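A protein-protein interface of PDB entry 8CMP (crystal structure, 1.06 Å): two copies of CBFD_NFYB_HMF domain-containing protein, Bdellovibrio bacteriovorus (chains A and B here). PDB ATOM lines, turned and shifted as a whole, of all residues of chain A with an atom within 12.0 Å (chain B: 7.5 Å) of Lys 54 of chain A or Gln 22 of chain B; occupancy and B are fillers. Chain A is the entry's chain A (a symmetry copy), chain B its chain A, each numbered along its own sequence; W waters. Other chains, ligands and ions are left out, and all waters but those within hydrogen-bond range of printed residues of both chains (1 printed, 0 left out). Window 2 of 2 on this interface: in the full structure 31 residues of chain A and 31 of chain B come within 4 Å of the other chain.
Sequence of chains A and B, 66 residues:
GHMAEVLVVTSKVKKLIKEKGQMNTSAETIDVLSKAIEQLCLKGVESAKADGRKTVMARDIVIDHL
No position is printed for both chains. Of the 13 pairs that touch across the chains among the printed residues, none has its exchanged pair printed and touching as well.
Among the printed residues, merely in contact across the chains: Cys 41 of chain A with Leu 16 of chain B (3.8 Å), Cys 41 of chain A with Ile 17 of chain B (3.9 Å), Val 45 of chain A with Gly 21 of chain B (3.8 Å), Lys 49 of chain A with Met 23 of chain B (3.7 Å), Lys 54 of chain A with Met 23 of chain B (3.4 Å), Thr 55 of chain A with Asn 24 of chain B (3.3 Å), Val 56 of chain A with Ile 17 of chain B (3.7 Å), Val 56 of chain A with Met 23 of chain B (3.9 Å) and Val 56 of chain A with Thr 25 of chain B (3.8 Å).
The backbone carbonyl oxygen of Ile 17 of chain B is in hydrogen-bond range of the backbone NH of Met 23 of chain B, at 3.5 Å. N of Lys 18 of chain B lies close to O of Met 23 of chain B (3.5 Å). OD1 of Asn 24 of chain B lies close to NZ of Lys 18 of chain B, 3.3 Å away. The backbone carbonyl oxygen (O) of Ala 48 of chain A lies within hydrogen-bond range of the backbone NH (N) of Arg 53 of chain A. OD2 of Asp 51 of chain A lies within salt-bridge range of NE of Arg 53 of chain A, 2.7 Å away. The guanidinium group (NH1) of Arg 53 of chain A lies within hydrogen-bond range of the backbone carbonyl oxygen (O) of Thr 55 of chain A.
NZ of Lys 54 of chain A sits at hydrogen-bond distance from O of Gln 22 of chain B, at 2.7 Å. The backbone NH (N) of Asn 24 of chain B lies within hydrogen-bond range of the backbone carbonyl oxygen (O) of Lys 54 of chain A (2.9 Å). The backbone carbonyl oxygen (O) of Asn 24 of chain B sits at hydrogen-bond distance from the backbone NH (N) of Val 56 of chain A (2.9 Å). O of Arg 53 of chain A sits close to SD of Met 23 of chain B (3.3 Å).
Water W1 lies within hydrogen-bond range of OE1 of Gln 22 of chain B (2.5 Å) and NZ of Lys 49 of chain A (3.0 Å).
Of the 11 printed residues of chain B, 7 touch a printed residue of chain A. Printed residues of chain B that touch a printed residue of chain A: Leu 16, Ile 17, Gly 21, Gln 22, Met 23, Asn 24 and Thr 25. Hydrophobic or aromatic side chains of chain B that line the printed part of chain A: Leu 16, Ile 17 and Met 23. Among the printed residues, no Asp or Glu carboxylate lies within 4 Å of a Lys or Arg side-chain nitrogen of the other chain.
Of chain A, only Lys 54 comes within 4 Å of Gln 22 of chain B. No residue of chain A comes within 4 Å of Lys 18 of chain B. Gly 21 of chain B touches one residue of chain A. Of the printed residues of chain A, Ile 17 of chain B touches Cys 41 and Val 56. Of the printed residues of chain B, Cys 41 of chain A touches Leu 16 and Ile 17. Of the printed residues of chain A, Thr 25 of chain B touches Val 56 (3.8 Å). The nearest residue of chain A that does not touch Gln 22 of chain B is Lys 49 of chain A (4.5 Å).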
ATOM      1  N   CYS A  41       8.578 -16.842  14.540  1.00  0.00           N
ATOM      2  CA  CYS A  41       8.334 -16.035  15.742  1.00  0.00           C
ATOM      3  C   CYS A  41       6.870 -15.637  15.849  1.00  0.00           C
ATOM      4  O   CYS A  41       6.280 -15.716  16.941  1.00  0.00           O
ATOM      5  CB  CYS A  41       9.207 -14.799  15.744  1.00  0.00           C
ATOM      6  SG  CYS A  41      10.954 -15.124  16.050  1.00  0.00           S
ATOM      7  N   LEU A  42       6.289 -15.192  14.745  1.00  0.00           N
ATOM      8  CA  LEU A  42       4.896 -14.748  14.794  1.00  0.00           C
ATOM      9  C   LEU A  42       3.982 -15.943  15.063  1.00  0.00           C
ATOM     10  O   LEU A  42       3.006 -15.796  15.819  1.00  0.00           O
ATOM     11  CB  LEU A  42       4.531 -14.022  13.507  1.00  0.00           C
ATOM     12  CG  LEU A  42       5.222 -12.700  13.273  1.00  0.00           C
ATOM     13  CD1 LEU A  42       4.931 -12.187  11.867  1.00  0.00           C
ATOM     14  CD2 LEU A  42       4.815 -11.680  14.316  1.00  0.00           C
ATOM     15  N   LYS A  43       4.232 -17.093  14.479  1.00  0.00           N
ATOM     16  CA  LYS A  43       3.434 -18.282  14.787  1.00  0.00           C
ATOM     17  C   LYS A  43       3.651 -18.665  16.239  1.00  0.00           C
ATOM     18  O   LYS A  43       2.717 -19.159  16.906  1.00  0.00           O
ATOM     19  CB  LYS A  43       3.783 -19.409  13.830  1.00  0.00           C
ATOM     20  CG  LYS A  43       3.280 -19.142  12.412  1.00  0.00           C
ATOM     21  CD  LYS A  43       3.556 -20.248  11.417  1.00  0.00           C
ATOM     22  CE  LYS A  43       3.184 -19.839  10.002  1.00  0.00           C
ATOM     23  NZ  LYS A  43       3.272 -20.959   9.039  1.00  0.00           N
ATOM     24  N   GLY A  44       4.848 -18.477  16.753  1.00  0.00           N
ATOM     25  CA  GLY A  44       5.120 -18.769  18.162  1.00  0.00           C
ATOM     26  C   GLY A  44       4.309 -17.874  19.086  1.00  0.00           C
ATOM     27  O   GLY A  44       3.801 -18.342  20.106  1.00  0.00           O
ATOM     28  N   VAL A  45       4.205 -16.609  18.761  1.00  0.00           N
ATOM     29  CA  VAL A  45       3.334 -15.688  19.520  1.00  0.00           C
ATOM     30  C   VAL A  45       1.926 -16.164  19.510  1.00  0.00           C
ATOM     31  O   VAL A  45       1.222 -16.225  20.524  1.00  0.00           O
ATOM     32  CB  VAL A  45       3.415 -14.288  18.939  1.00  0.00           C
ATOM     33  CG1 VAL A  45       2.283 -13.407  19.449  1.00  0.00           C
ATOM     34  CG2 VAL A  45       4.748 -13.663  19.238  1.00  0.00           C
ATOM     35  N   GLU A  46       1.391 -16.615  18.369  1.00  0.00           N
ATOM     36  CA  GLU A  46      -0.003 -17.133  18.234  1.00  0.00           C
ATOM     37  C   GLU A  46      -0.177 -18.289  19.195  1.00  0.00           C
ATOM     38  O   GLU A  46      -1.181 -18.360  19.911  1.00  0.00           O
ATOM     39  CB  GLU A  46      -0.333 -17.554  16.794  1.00  0.00           C
ATOM     40  CG  GLU A  46      -0.346 -16.396  15.801  1.00  0.00           C
ATOM     41  CD  GLU A  46      -1.418 -15.391  16.118  1.00  0.00           C
ATOM     42  OE1 GLU A  46      -2.611 -15.780  16.021  1.00  0.00           O
ATOM     43  OE2 GLU A  46      -1.089 -14.253  16.502  1.00  0.00           O
ATOM     44  N   SER A  47       0.763 -19.234  19.157  1.00  0.00           N
ATOM     45  CA  SER A  47       0.646 -20.463  19.970  1.00  0.00           C
ATOM     46  C   SER A  47       0.705 -20.119  21.464  1.00  0.00           C
ATOM     47  O   SER A  47      -0.088 -20.635  22.264  1.00  0.00           O
ATOM     48  CB  SER A  47       1.794 -21.404  19.587  1.00  0.00           C
ATOM     49  OG  SER A  47       1.903 -22.515  20.438  1.00  0.00           O
ATOM     50  N   ALA A  48       1.643 -19.284  21.851  1.00  0.00           N
ATOM     51  CA  ALA A  48       1.800 -18.933  23.276  1.00  0.00           C
ATOM     52  C   ALA A  48       0.589 -18.209  23.800  1.00  0.00           C
ATOM     53  O   ALA A  48       0.085 -18.517  24.886  1.00  0.00           O
ATOM     54  CB  ALA A  48       3.062 -18.111  23.460  1.00  0.00           C
ATOM     55  N   LYS A  49       0.071 -17.260  23.017  1.00  0.00           N
ATOM     56  CA  LYS A  49      -1.095 -16.516  23.452  1.00  0.00           C
ATOM     57  C   LYS A  49      -2.311 -17.424  23.520  1.00  0.00           C
ATOM     58  O   LYS A  49      -3.139 -17.272  24.443  1.00  0.00           O
ATOM     59  CB  LYS A  49      -1.358 -15.335  22.550  1.00  0.00           C
ATOM     60  CG  LYS A  49      -0.341 -14.246  22.678  1.00  0.00           C
ATOM     61  CD  LYS A  49      -0.742 -12.973  21.996  1.00  0.00           C
ATOM     62  CE  LYS A  49      -1.800 -12.256  22.810  1.00  0.00           C
ATOM     63  NZ  LYS A  49      -2.283 -10.979  22.222  1.00  0.00           N
ATOM     64  N   ALA A  50      -2.476 -18.317  22.578  1.00  0.00           N
ATOM     65  CA  ALA A  50      -3.632 -19.239  22.603  1.00  0.00           C
ATOM     66  C   ALA A  50      -3.580 -20.081  23.880  1.00  0.00           C
ATOM     67  O   ALA A  50      -4.629 -20.516  24.325  1.00  0.00           O
ATOM     68  CB  ALA A  50      -3.605 -20.115  21.372  1.00  0.00           C
ATOM     69  N   ASP A  51      -2.397 -20.363  24.406  1.00  0.00           N
ATOM     70  CA  ASP A  51      -2.190 -21.168  25.624  1.00  0.00           C
ATOM     71  C   ASP A  51      -2.291 -20.255  26.855  1.00  0.00           C
ATOM     72  O   ASP A  51      -2.093 -20.763  27.956  1.00  0.00           O
ATOM     73  CB  ASP A  51      -0.873 -21.932  25.585  1.00  0.00           C
ATOM     74  CG  ASP A  51      -0.796 -23.136  26.527  1.00  0.00           C
ATOM     75  OD1 ASP A  51      -1.791 -23.854  26.621  1.00  0.00           O
ATOM     76  OD2 ASP A  51       0.246 -23.341  27.159  1.00  0.00           O
ATOM     77  N   GLY A  52      -2.569 -18.956  26.739  1.00  0.00           N
ATOM     78  CA  GLY A  52      -2.672 -18.010  27.871  1.00  0.00           C
ATOM     79  C   GLY A  52      -1.356 -17.688  28.519  1.00  0.00           C
ATOM     80  O   GLY A  52      -1.323 -17.249  29.661  1.00  0.00           O
ATOM     81  N   ARG A  53      -0.268 -17.827  27.769  1.00  0.00           N
ATOM     82  CA  ARG A  53       1.068 -17.567  28.318  1.00  0.00           C
ATOM     83  C   ARG A  53       1.564 -16.192  27.878  1.00  0.00           C
ATOM     84  O   ARG A  53       1.036 -15.627  26.910  1.00  0.00           O
ATOM     85  CB  ARG A  53       2.045 -18.663  27.923  1.00  0.00           C
ATOM     86  CG  ARG A  53       1.831 -19.919  28.740  1.00  0.00           C
ATOM     87  CD  ARG A  53       2.804 -21.007  28.339  1.00  0.00           C
ATOM     88  NE  ARG A  53       2.418 -21.666  27.110  1.00  0.00           N
ATOM     89  CZ  ARG A  53       3.035 -21.556  25.948  1.00  0.00           C
ATOM     90  NH1 ARG A  53       4.031 -20.696  25.758  1.00  0.00           N
ATOM     91  NH2 ARG A  53       2.645 -22.350  24.964  1.00  0.00           N
ATOM     92  N   LYS A  54       2.591 -15.712  28.579  1.00  0.00           N
ATOM     93  CA  LYS A  54       3.250 -14.421  28.287  1.00  0.00           C
ATOM     94  C   LYS A  54       4.669 -14.592  27.787  1.00  0.00           C
ATOM     95  O   LYS A  54       5.351 -13.607  27.640  1.00  0.00           O
ATOM     96  CB  LYS A  54       3.185 -13.560  29.539  1.00  0.00           C
ATOM     97  CG  LYS A  54       1.756 -13.158  29.848  1.00  0.00           C
ATOM     98  CD  LYS A  54       1.158 -12.185  28.827  1.00  0.00           C
ATOM     99  CE  LYS A  54       1.761 -10.793  28.869  1.00  0.00           C
ATOM    100  NZ  LYS A  54       1.594 -10.077  27.581  1.00  0.00           N
ATOM    101  N   THR A  55       5.087 -15.835  27.537  1.00  0.00           N
ATOM    102  CA  THR A  55       6.429 -16.140  27.030  1.00  0.00           C
ATOM    103  C   THR A  55       6.288 -17.136  25.897  1.00  0.00           C
ATOM    104  O   THR A  55       5.617 -18.144  26.056  1.00  0.00           O
ATOM    105  CB  THR A  55       7.299 -16.734  28.142  1.00  0.00           C
ATOM    106  OG1 THR A  55       7.352 -15.808  29.226  1.00  0.00           O
ATOM    107  CG2 THR A  55       8.706 -17.024  27.714  1.00  0.00           C
ATOM    108  N   VAL A  56       6.967 -16.843  24.786  1.00  0.00           N
ATOM    109  CA  VAL A  56       7.110 -17.788  23.685  1.00  0.00           C
ATOM    110  C   VAL A  56       8.200 -18.788  24.073  1.00  0.00           C
ATOM    111  O   VAL A  56       9.344 -18.387  24.355  1.00  0.00           O
ATOM    112  CB  VAL A  56       7.457 -17.055  22.389  1.00  0.00           C
ATOM    113  CG1 VAL A  56       7.707 -18.036  21.270  1.00  0.00           C
ATOM    114  CG2 VAL A  56       6.365 -16.087  22.018  1.00  0.00           C
ATOM    115  N   MET A  57       7.836 -20.038  24.028  1.00  0.00           N
ATOM    116  CA  MET A  57       8.662 -21.174  24.461  1.00  0.00           C
ATOM    117  C   MET A  57       9.053 -22.022  23.257  1.00  0.00           C
ATOM    118  O   MET A  57       8.517 -21.867  22.149  1.00  0.00           O
ATOM    119  CB  MET A  57       7.860 -22.035  25.423  1.00  0.00           C
ATOM    120  CG  MET A  57       7.420 -21.278  26.600  1.00  0.00           C
ATOM    121  SD  MET A  57       6.640 -22.218  27.859  1.00  0.00           S
ATOM    122  CE  MET A  57       6.561 -20.900  29.053  1.00  0.00           C
ATOM    123  N   ALA A  58      10.003 -22.919  23.458  1.00  0.00           N
ATOM    124  CA  ALA A  58      10.437 -23.781  22.370  1.00  0.00           C
ATOM    125  C   ALA A  58       9.277 -24.569  21.789  1.00  0.00           C
ATOM    126  O   ALA A  58       9.249 -24.782  20.581  1.00  0.00           O
ATOM    127  CB  ALA A  58      11.535 -24.683  22.830  1.00  0.00           C
ATOM    128  N   ARG A  59       8.345 -25.027  22.601  1.00  0.00           N
ATOM    129  CA  ARG A  59       7.215 -25.842  22.089  1.00  0.00           C
ATOM    130  C   ARG A  59       6.306 -24.994  21.208  1.00  0.00           C
ATOM    131  O   ARG A  59       5.496 -25.581  20.508  1.00  0.00           O
ATOM    132  CB  ARG A  59       6.441 -26.480  23.234  1.00  0.00           C
ATOM    133  CG  ARG A  59       5.657 -25.580  24.148  1.00  0.00           C
ATOM    134  CD  ARG A  59       4.733 -26.469  25.021  1.00  0.00           C
ATOM    135  NE  ARG A  59       3.851 -25.747  25.902  1.00  0.00           N
ATOM    136  CZ  ARG A  59       4.179 -25.333  27.098  1.00  0.00           C
ATOM    137  NH1 ARG A  59       5.387 -25.548  27.537  1.00  0.00           N
ATOM    138  NH2 ARG A  59       3.270 -24.725  27.839  1.00  0.00           N
ATOM    139  N   ASP A  60       6.426 -23.666  21.232  1.00  0.00           N
ATOM    140  CA  ASP A  60       5.625 -22.796  20.341  1.00  0.00           C
ATOM    141  C   ASP A  60       6.220 -22.657  18.953  1.00  0.00           C
ATOM    142  O   ASP A  60       5.567 -22.072  18.085  1.00  0.00           O
ATOM    143  CB  ASP A  60       5.511 -21.429  20.991  1.00  0.00           C
ATOM    144  CG  ASP A  60       4.762 -21.452  22.352  1.00  0.00           C
ATOM    145  OD1 ASP A  60       3.685 -22.094  22.403  1.00  0.00           O
ATOM    146  OD2 ASP A  60       5.263 -20.810  23.316  1.00  0.00           O
ATOM    147  N   LYS B  15      13.003  -8.486  20.415  1.00  0.00           N
ATOM    148  CA  LYS B  15      12.306  -7.226  20.117  1.00  0.00           C
ATOM    149  C   LYS B  15      11.052  -7.501  19.306  1.00  0.00           C
ATOM    150  O   LYS B  15       9.988  -6.931  19.582  1.00  0.00           O
ATOM    151  CB  LYS B  15      13.235  -6.293  19.353  1.00  0.00           C
ATOM    152  CG  LYS B  15      12.623  -5.003  18.840  1.00  0.00           C
ATOM    153  CD  LYS B  15      13.652  -4.146  18.107  1.00  0.00           C
ATOM    154  CE  LYS B  15      13.168  -2.769  17.751  1.00  0.00           C
ATOM    155  NZ  LYS B  15      12.351  -2.790  16.516  1.00  0.00           N
ATOM    156  N   LEU B  16      11.172  -8.307  18.250  1.00  0.00           N
ATOM    157  CA  LEU B  16      10.010  -8.629  17.387  1.00  0.00           C
ATOM    158  C   LEU B  16       8.879  -9.255  18.244  1.00  0.00           C
ATOM    159  O   LEU B  16       7.726  -8.831  18.167  1.00  0.00           O
ATOM    160  CB  LEU B  16      10.451  -9.621  16.307  1.00  0.00           C
ATOM    161  CG  LEU B  16       9.337 -10.155  15.392  1.00  0.00           C
ATOM    162  CD1 LEU B  16       8.725  -9.039  14.580  1.00  0.00           C
ATOM    163  CD2 LEU B  16       9.855 -11.262  14.505  1.00  0.00           C
ATOM    164  N   ILE B  17       9.232 -10.231  19.069  1.00  0.00           N
ATOM    165  CA  ILE B  17       8.226 -10.948  19.854  1.00  0.00           C
ATOM    166  C   ILE B  17       7.585 -10.007  20.884  1.00  0.00           C
ATOM    167  O   ILE B  17       6.367 -10.084  21.097  1.00  0.00           O
ATOM    168  CB  ILE B  17       8.857 -12.215  20.432  1.00  0.00           C
ATOM    169  CG1 ILE B  17       9.091 -13.225  19.309  1.00  0.00           C
ATOM    170  CG2 ILE B  17       8.030 -12.785  21.538  1.00  0.00           C
ATOM    171  CD1 ILE B  17       9.892 -14.440  19.753  1.00  0.00           C
ATOM    172  N   LYS B  18       8.366  -9.132  21.474  1.00  0.00           N
ATOM    173  CA  LYS B  18       7.827  -8.202  22.482  1.00  0.00           C
ATOM    174  C   LYS B  18       6.936  -7.156  21.820  1.00  0.00           C
ATOM    175  O   LYS B  18       5.810  -6.847  22.310  1.00  0.00           O
ATOM    176  CB  LYS B  18       8.945  -7.566  23.275  1.00  0.00           C
ATOM    177  CG  LYS B  18       8.401  -6.817  24.473  1.00  0.00           C
ATOM    178  CD  LYS B  18       7.552  -7.582  25.458  1.00  0.00           C
ATOM    179  CE  LYS B  18       8.421  -8.411  26.363  1.00  0.00           C
ATOM    180  NZ  LYS B  18       9.138  -7.587  27.350  1.00  0.00           N
ATOM    181  N   GLU B  19       7.387  -6.575  20.739  1.00  0.00           N
ATOM    182  CA  GLU B  19       6.654  -5.462  20.119  1.00  0.00           C
ATOM    183  C   GLU B  19       5.398  -5.970  19.404  1.00  0.00           C
ATOM    184  O   GLU B  19       4.386  -5.288  19.413  1.00  0.00           O
ATOM    185  CB  GLU B  19       7.611  -4.645  19.260  1.00  0.00           C
ATOM    186  CG  GLU B  19       8.619  -3.910  20.141  1.00  0.00           C
ATOM    187  CD  GLU B  19       9.542  -2.910  19.503  1.00  0.00           C
ATOM    188  OE1 GLU B  19       9.633  -2.929  18.223  1.00  0.00           O
ATOM    189  OE2 GLU B  19      10.284  -2.221  20.288  1.00  0.00           O
ATOM    190  N   LYS B  20       5.458  -7.147  18.789  1.00  0.00           N
ATOM    191  CA  LYS B  20       4.313  -7.699  18.030  1.00  0.00           C
ATOM    192  C   LYS B  20       3.360  -8.473  18.934  1.00  0.00           C
ATOM    193  O   LYS B  20       2.149  -8.492  18.570  1.00  0.00           O
ATOM    194  CB  LYS B  20       4.772  -8.626  16.909  1.00  0.00           C
ATOM    195  CG  LYS B  20       5.462  -7.893  15.783  1.00  0.00           C
ATOM    196  CD  LYS B  20       4.512  -7.553  14.696  1.00  0.00           C
ATOM    197  CE  LYS B  20       5.168  -6.773  13.577  1.00  0.00           C
ATOM    198  NZ  LYS B  20       5.150  -5.315  13.842  1.00  0.00           N
ATOM    199  N   GLY B  21       3.827  -9.130  20.012  1.00  0.00           N
ATOM    200  CA  GLY B  21       2.973  -9.942  20.924  1.00  0.00           C
ATOM    201  C   GLY B  21       2.934  -9.539  22.396  1.00  0.00           C
ATOM    202  O   GLY B  21       2.201 -10.247  23.177  1.00  0.00           O
ATOM    203  N   GLN B  22       3.687  -8.570  22.805  1.00  0.00           N
ATOM    204  CA  GLN B  22       3.874  -8.245  24.255  1.00  0.00           C
ATOM    205  C   GLN B  22       4.272  -9.527  24.965  1.00  0.00           C
ATOM    206  O   GLN B  22       3.833  -9.733  26.081  1.00  0.00           O
ATOM    207  CB  GLN B  22       2.637  -7.665  24.920  1.00  0.00           C
ATOM    208  CG  GLN B  22       2.144  -6.428  24.234  1.00  0.00           C
ATOM    209  CD  GLN B  22       1.454  -6.717  22.931  1.00  0.00           C
ATOM    210  OE1 GLN B  22       0.553  -7.547  22.854  1.00  0.00           O
ATOM    211  NE2 GLN B  22       1.864  -6.009  21.903  1.00  0.00           N
ATOM    212  N   MET B  23       5.079 -10.356  24.312  1.00  0.00           N
ATOM    213  CA  MET B  23       5.500 -11.657  24.829  1.00  0.00           C
ATOM    214  C   MET B  23       7.014 -11.467  25.177  1.00  0.00           C
ATOM    215  O   MET B  23       7.806 -10.865  24.453  1.00  0.00           O
ATOM    216  CB  MET B  23       5.248 -12.823  23.804  1.00  0.00           C
ATOM    217  CG  MET B  23       3.790 -13.428  23.363  1.00  0.00           C
ATOM    218  SD  MET B  23       2.842 -14.056  24.663  1.00  0.00           S
ATOM    219  CE  MET B  23       1.934 -12.578  25.090  1.00  0.00           C
ATOM    220  N   ASN B  24       7.418 -12.177  26.201  1.00  0.00           N
ATOM    221  CA  ASN B  24       8.831 -12.527  26.451  1.00  0.00           C
ATOM    222  C   ASN B  24       9.245 -13.725  25.576  1.00  0.00           C
ATOM    223  O   ASN B  24       8.385 -14.367  24.977  1.00  0.00           O
ATOM    224  CB  ASN B  24       9.027 -12.896  27.910  1.00  0.00           C
ATOM    225  CG  ASN B  24       8.693 -11.736  28.810  1.00  0.00           C
ATOM    226  OD1 ASN B  24       9.168 -10.626  28.593  1.00  0.00           O
ATOM    227  ND2 ASN B  24       7.840 -11.999  29.773  1.00  0.00           N
ATOM    228  N   THR B  25      10.553 -13.958  25.500  1.00  0.00           N
ATOM    229  CA  THR B  25      11.157 -15.028  24.685  1.00  0.00           C
ATOM    230  C   THR B  25      12.032 -15.877  25.574  1.00  0.00           C
ATOM    231  O   THR B  25      12.984 -15.356  26.121  1.00  0.00           O
ATOM    232  CB  THR B  25      11.966 -14.433  23.525  1.00  0.00           C
ATOM    233  OG1 THR B  25      11.167 -13.580  22.749  1.00  0.00           O
ATOM    234  CG2 THR B  25      12.483 -15.519  22.618  1.00  0.00           C
HETATM  235  O   HOH W   1      -0.327  -9.032  21.053  1.00  0.00           O
